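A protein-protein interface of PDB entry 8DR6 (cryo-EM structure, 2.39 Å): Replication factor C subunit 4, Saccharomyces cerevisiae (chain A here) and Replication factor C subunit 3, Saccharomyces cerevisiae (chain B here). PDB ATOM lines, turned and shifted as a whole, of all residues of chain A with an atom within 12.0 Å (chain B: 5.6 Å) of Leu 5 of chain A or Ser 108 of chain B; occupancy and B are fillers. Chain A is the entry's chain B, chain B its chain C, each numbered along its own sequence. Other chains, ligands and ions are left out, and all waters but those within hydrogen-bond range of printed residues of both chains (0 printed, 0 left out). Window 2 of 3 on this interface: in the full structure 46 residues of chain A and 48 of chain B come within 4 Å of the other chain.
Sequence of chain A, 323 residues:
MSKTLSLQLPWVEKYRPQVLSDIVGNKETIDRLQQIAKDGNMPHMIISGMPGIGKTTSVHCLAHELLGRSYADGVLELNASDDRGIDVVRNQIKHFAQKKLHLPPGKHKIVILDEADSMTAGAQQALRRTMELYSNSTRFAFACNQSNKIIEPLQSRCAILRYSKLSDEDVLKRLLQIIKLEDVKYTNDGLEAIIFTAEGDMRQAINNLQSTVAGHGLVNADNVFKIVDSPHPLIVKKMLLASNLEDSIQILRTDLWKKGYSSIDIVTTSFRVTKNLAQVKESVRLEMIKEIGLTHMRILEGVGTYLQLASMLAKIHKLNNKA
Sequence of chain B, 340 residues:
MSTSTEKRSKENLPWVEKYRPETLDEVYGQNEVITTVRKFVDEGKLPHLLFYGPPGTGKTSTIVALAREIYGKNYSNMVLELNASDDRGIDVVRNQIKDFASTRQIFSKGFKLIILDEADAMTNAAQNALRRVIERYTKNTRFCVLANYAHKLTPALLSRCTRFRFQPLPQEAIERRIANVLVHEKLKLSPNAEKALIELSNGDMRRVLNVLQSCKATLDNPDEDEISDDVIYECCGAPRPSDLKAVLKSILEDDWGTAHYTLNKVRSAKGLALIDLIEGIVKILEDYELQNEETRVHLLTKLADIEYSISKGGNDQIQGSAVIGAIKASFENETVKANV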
ATOM      1  N   THR A   4      32.933  -9.977  24.615  1.00  0.00           N
ATOM      2  CA  THR A   4      31.520  -9.671  24.800  1.00  0.00           C
ATOM      3  C   THR A   4      30.685 -10.918  24.522  1.00  0.00           C
ATOM      4  O   THR A   4      30.911 -11.623  23.538  1.00  0.00           O
ATOM      5  CB  THR A   4      31.074  -8.508  23.883  1.00  0.00           C
ATOM      6  OG1 THR A   4      31.233  -7.263  24.576  1.00  0.00           O
ATOM      7  CG2 THR A   4      29.615  -8.657  23.460  1.00  0.00           C
ATOM      8  N   LEU A   5      29.715 -11.183  25.398  1.00  0.00           N
ATOM      9  CA  LEU A   5      28.876 -12.371  25.320  1.00  0.00           C
ATOM     10  C   LEU A   5      27.508 -12.068  24.712  1.00  0.00           C
ATOM     11  O   LEU A   5      26.499 -12.651  25.115  1.00  0.00           O
ATOM     12  CB  LEU A   5      28.712 -12.996  26.705  1.00  0.00           C
ATOM     13  CG  LEU A   5      29.996 -13.477  27.386  1.00  0.00           C
ATOM     14  CD1 LEU A   5      29.683 -14.069  28.751  1.00  0.00           C
ATOM     15  CD2 LEU A   5      30.729 -14.491  26.519  1.00  0.00           C
ATOM     16  N   SER A   6      27.464 -11.160  23.743  1.00  0.00           N
ATOM     17  CA  SER A   6      26.236 -10.789  23.057  1.00  0.00           C
ATOM     18  C   SER A   6      26.406 -10.973  21.554  1.00  0.00           C
ATOM     19  O   SER A   6      27.499 -10.809  21.005  1.00  0.00           O
ATOM     20  CB  SER A   6      25.850  -9.338  23.368  1.00  0.00           C
ATOM     21  OG  SER A   6      26.281  -8.465  22.339  1.00  0.00           O
ATOM     22  N   LEU A   7      25.304 -11.316  20.893  1.00  0.00           N
ATOM     23  CA  LEU A   7      25.297 -11.586  19.462  1.00  0.00           C
ATOM     24  C   LEU A   7      24.251 -10.714  18.787  1.00  0.00           C
ATOM     25  O   LEU A   7      23.108 -10.641  19.247  1.00  0.00           O
ATOM     26  CB  LEU A   7      25.005 -13.066  19.178  1.00  0.00           C
ATOM     27  CG  LEU A   7      26.131 -14.066  19.449  1.00  0.00           C
ATOM     28  CD1 LEU A   7      25.684 -15.470  19.076  1.00  0.00           C
ATOM     29  CD2 LEU A   7      27.399 -13.692  18.695  1.00  0.00           C
ATOM     30  N   GLN A   8      24.648 -10.056  17.701  1.00  0.00           N
ATOM     31  CA  GLN A   8      23.711  -9.290  16.893  1.00  0.00           C
ATOM     32  C   GLN A   8      22.992 -10.214  15.921  1.00  0.00           C
ATOM     33  O   GLN A   8      23.617 -11.043  15.252  1.00  0.00           O
ATOM     34  CB  GLN A   8      24.441  -8.185  16.130  1.00  0.00           C
ATOM     35  CG  GLN A   8      23.537  -7.329  15.256  1.00  0.00           C
ATOM     36  CD  GLN A   8      24.269  -6.156  14.635  1.00  0.00           C
ATOM     37  OE1 GLN A   8      24.729  -6.228  13.496  1.00  0.00           O
ATOM     38  NE2 GLN A   8      24.382  -5.065  15.384  1.00  0.00           N
ATOM     39  N   LEU A   9      21.676 -10.072  15.846  1.00  0.00           N
ATOM     40  CA  LEU A   9      20.884 -10.953  14.998  1.00  0.00           C
ATOM     41  C   LEU A   9      21.285 -10.761  13.538  1.00  0.00           C
ATOM     42  O   LEU A   9      21.312  -9.623  13.055  1.00  0.00           O
ATOM     43  CB  LEU A   9      19.395 -10.668  15.182  1.00  0.00           C
ATOM     44  CG  LEU A   9      18.435 -11.573  14.408  1.00  0.00           C
ATOM     45  CD1 LEU A   9      18.402 -12.965  15.019  1.00  0.00           C
ATOM     46  CD2 LEU A   9      17.040 -10.970  14.377  1.00  0.00           C
ATOM     47  N   ILE B  70      36.835 -15.025  24.165  1.00  0.00           N
ATOM     48  CA  ILE B  70      35.410 -14.778  24.362  1.00  0.00           C
ATOM     49  C   ILE B  70      34.958 -15.258  25.736  1.00  0.00           C
ATOM     50  O   ILE B  70      34.211 -14.562  26.432  1.00  0.00           O
ATOM     51  CB  ILE B  70      34.597 -15.441  23.236  1.00  0.00           C
ATOM     52  CG1 ILE B  70      34.823 -14.708  21.913  1.00  0.00           C
ATOM     53  CG2 ILE B  70      33.115 -15.454  23.587  1.00  0.00           C
ATOM     54  CD1 ILE B  70      34.489 -15.537  20.692  1.00  0.00           C
ATOM     55  N   TYR B  71      35.397 -16.445  26.147  1.00  0.00           N
ATOM     56  CA  TYR B  71      34.949 -17.064  27.390  1.00  0.00           C
ATOM     57  C   TYR B  71      35.967 -16.979  28.514  1.00  0.00           C
ATOM     58  O   TYR B  71      35.597 -16.672  29.649  1.00  0.00           O
ATOM     59  CB  TYR B  71      34.597 -18.536  27.145  1.00  0.00           C
ATOM     60  CG  TYR B  71      33.499 -18.735  26.125  1.00  0.00           C
ATOM     61  CD1 TYR B  71      32.181 -18.419  26.425  1.00  0.00           C
ATOM     62  CD2 TYR B  71      33.780 -19.236  24.861  1.00  0.00           C
ATOM     63  CE1 TYR B  71      31.174 -18.598  25.496  1.00  0.00           C
ATOM     64  CE2 TYR B  71      32.780 -19.418  23.926  1.00  0.00           C
ATOM     65  CZ  TYR B  71      31.479 -19.097  24.248  1.00  0.00           C
ATOM     66  OH  TYR B  71      30.480 -19.277  23.320  1.00  0.00           O
ATOM     67  N   MET B  78      32.635 -24.608  27.557  1.00  0.00           N
ATOM     68  CA  MET B  78      31.607 -23.738  27.006  1.00  0.00           C
ATOM     69  C   MET B  78      31.487 -23.835  25.492  1.00  0.00           C
ATOM     70  O   MET B  78      30.582 -23.217  24.919  1.00  0.00           O
ATOM     71  CB  MET B  78      31.891 -22.282  27.397  1.00  0.00           C
ATOM     72  CG  MET B  78      32.330 -22.116  28.842  1.00  0.00           C
ATOM     73  SD  MET B  78      32.164 -20.430  29.456  1.00  0.00           S
ATOM     74  CE  MET B  78      30.388 -20.227  29.421  1.00  0.00           C
ATOM     75  N   GLN B 105      23.807 -22.094  28.187  1.00  0.00           N
ATOM     76  CA  GLN B 105      25.089 -22.398  28.804  1.00  0.00           C
ATOM     77  C   GLN B 105      24.907 -22.718  30.284  1.00  0.00           C
ATOM     78  O   GLN B 105      24.116 -22.085  30.989  1.00  0.00           O
ATOM     79  CB  GLN B 105      26.052 -21.222  28.645  1.00  0.00           C
ATOM     80  CG  GLN B 105      26.461 -20.939  27.210  1.00  0.00           C
ATOM     81  CD  GLN B 105      27.762 -21.617  26.830  1.00  0.00           C
ATOM     82  OE1 GLN B 105      28.151 -22.619  27.429  1.00  0.00           O
ATOM     83  NE2 GLN B 105      28.442 -21.072  25.829  1.00  0.00           N
ATOM     84  N   ILE B 106      25.654 -23.717  30.754  1.00  0.00           N
ATOM     85  CA  ILE B 106      25.584 -24.093  32.161  1.00  0.00           C
ATOM     86  C   ILE B 106      26.222 -23.025  33.041  1.00  0.00           C
ATOM     87  O   ILE B 106      25.658 -22.638  34.071  1.00  0.00           O
ATOM     88  CB  ILE B 106      26.246 -25.467  32.379  1.00  0.00           C
ATOM     89  CG1 ILE B 106      25.572 -26.535  31.513  1.00  0.00           C
ATOM     90  CG2 ILE B 106      26.185 -25.858  33.850  1.00  0.00           C
ATOM     91  CD1 ILE B 106      26.349 -27.832  31.428  1.00  0.00           C
ATOM     92  N   PHE B 107      27.398 -22.533  32.656  1.00  0.00           N
ATOM     93  CA  PHE B 107      28.166 -21.638  33.514  1.00  0.00           C
ATOM     94  C   PHE B 107      27.714 -20.188  33.388  1.00  0.00           C
ATOM     95  O   PHE B 107      27.236 -19.597  34.362  1.00  0.00           O
ATOM     96  CB  PHE B 107      29.656 -21.753  33.189  1.00  0.00           C
ATOM     97  CG  PHE B 107      30.208 -23.139  33.368  1.00  0.00           C
ATOM     98  CD1 PHE B 107      30.086 -24.083  32.362  1.00  0.00           C
ATOM     99  CD2 PHE B 107      30.843 -23.500  34.544  1.00  0.00           C
ATOM    100  CE1 PHE B 107      30.590 -25.359  32.525  1.00  0.00           C
ATOM    101  CE2 PHE B 107      31.349 -24.774  34.712  1.00  0.00           C
ATOM    102  CZ  PHE B 107      31.223 -25.705  33.702  1.00  0.00           C
ATOM    103  N   SER B 108      27.855 -19.608  32.199  1.00  0.00           N
ATOM    104  CA  SER B 108      27.560 -18.197  31.990  1.00  0.00           C
ATOM    105  C   SER B 108      26.216 -18.058  31.274  1.00  0.00           C
ATOM    106  O   SER B 108      25.496 -19.040  31.074  1.00  0.00           O
ATOM    107  CB  SER B 108      28.701 -17.536  31.213  1.00  0.00           C
ATOM    108  OG  SER B 108      28.533 -17.712  29.816  1.00  0.00           O
ATOM    109  N   LYS B 109      25.865 -16.831  30.884  1.00  0.00           N
ATOM    110  CA  LYS B 109      24.626 -16.547  30.169  1.00  0.00           C
ATOM    111  C   LYS B 109      24.889 -16.104  28.733  1.00  0.00           C
ATOM    112  O   LYS B 109      24.009 -15.512  28.099  1.00  0.00           O
ATOM    113  CB  LYS B 109      23.821 -15.478  30.912  1.00  0.00           C
ATOM    114  CG  LYS B 109      23.434 -15.867  32.333  1.00  0.00           C
ATOM    115  CD  LYS B 109      23.450 -14.671  33.279  1.00  0.00           C
ATOM    116  CE  LYS B 109      22.236 -13.771  33.089  1.00  0.00           C
ATOM    117  NZ  LYS B 109      22.252 -13.046  31.788  1.00  0.00           N
ATOM    118  N   GLY B 110      26.084 -16.379  28.207  1.00  0.00           N
ATOM    119  CA  GLY B 110      26.451 -15.946  26.877  1.00  0.00           C
ATOM    120  C   GLY B 110      26.013 -16.921  25.798  1.00  0.00           C
ATOM    121  O   GLY B 110      25.324 -17.909  26.043  1.00  0.00           O
ATOM    122  N   PHE B 111      26.434 -16.620  24.572  1.00  0.00           N
ATOM    123  CA  PHE B 111      26.108 -17.469  23.438  1.00  0.00           C
ATOM    124  C   PHE B 111      26.989 -18.718  23.442  1.00  0.00           C
ATOM    125  O   PHE B 111      27.866 -18.897  24.291  1.00  0.00           O
ATOM    126  CB  PHE B 111      26.264 -16.696  22.128  1.00  0.00           C
ATOM    127  CG  PHE B 111      27.688 -16.356  21.783  1.00  0.00           C
ATOM    128  CD1 PHE B 111      28.470 -17.238  21.056  1.00  0.00           C
ATOM    129  CD2 PHE B 111      28.241 -15.151  22.181  1.00  0.00           C
ATOM    130  CE1 PHE B 111      29.777 -16.926  20.737  1.00  0.00           C
ATOM    131  CE2 PHE B 111      29.547 -14.833  21.864  1.00  0.00           C
ATOM    132  CZ  PHE B 111      30.316 -15.721  21.141  1.00  0.00           C
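The side-chain hydroxyl (OG) of Ser 108 of chain B lies within hydrogen-bond range of the backbone NH (N) of Gly 110 of chain B, at 3.2 Å. NE2 of Gln 105 of chain B lies within hydrogen-bond range of O of Phe 111 of chain B (2.7 Å). The side-chain hydroxyl (OH) of Tyr 71 of chain B sits at hydrogen-bond distance from the backbone carbonyl oxygen (O) of Phe 111 of chain B (2.8 Å).
Phe 111 of chain B touches Thr 4 of chain A (CE2 to O, 3.9 Å). O of Ile 70 of chain B touches CD2 of Leu 5 of chain A, at 3.5 Å. Leu 5 of chain A touches Ser 108 of chain B (CD1 to OG, 3.97 Å). CA of Gly 110 of chain B touches CB of Leu 5 of chain A (3.7 Å). Phe 111 of chain B touches Leu 7 of chain A (CB to CD1, 3.3 Å).
Printed residues of chain B within 4 Å of Thr 4 of chain A: Phe 111 (3.9 Å). Of the printed residues of chain B, Leu 5 of chain A touches Ile 70 (3.5 Å), Ser 108 (3.97 Å) and Gly 110 (3.7 Å). Ser 6 of chain A touches none of the printed residues of chain B. Of the printed residues of chain B, Leu 7 of chain A touches Phe 111. Ile 106 of chain B touches none of the printed residues of chain A. Of the printed residues of chain A, Ser 108 of chain B touches Leu 5 (3.97 Å). No residue of chain A comes within 4 Å of Lys 109 of chain B. Gly 110 of chain B touches one residue of chain A. Of the printed residues of chain A, Phe 111 of chain B touches Thr 4 (3.9 Å) and Leu 7 (3.3 Å). The nearest printed residue of chain B that does not touch Leu 5 of chain A is Phe 111 of chain B (4.01 Å).
Printed residues of chain A that touch a printed residue of chain B: Thr 4, Leu 5 and Leu 7. Hydrophobic or aromatic side chains of chain A within 4 Å of the printed part of chain B: Leu 5 and Leu 7. Among the printed residues, 5 pairs touch across the chains.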
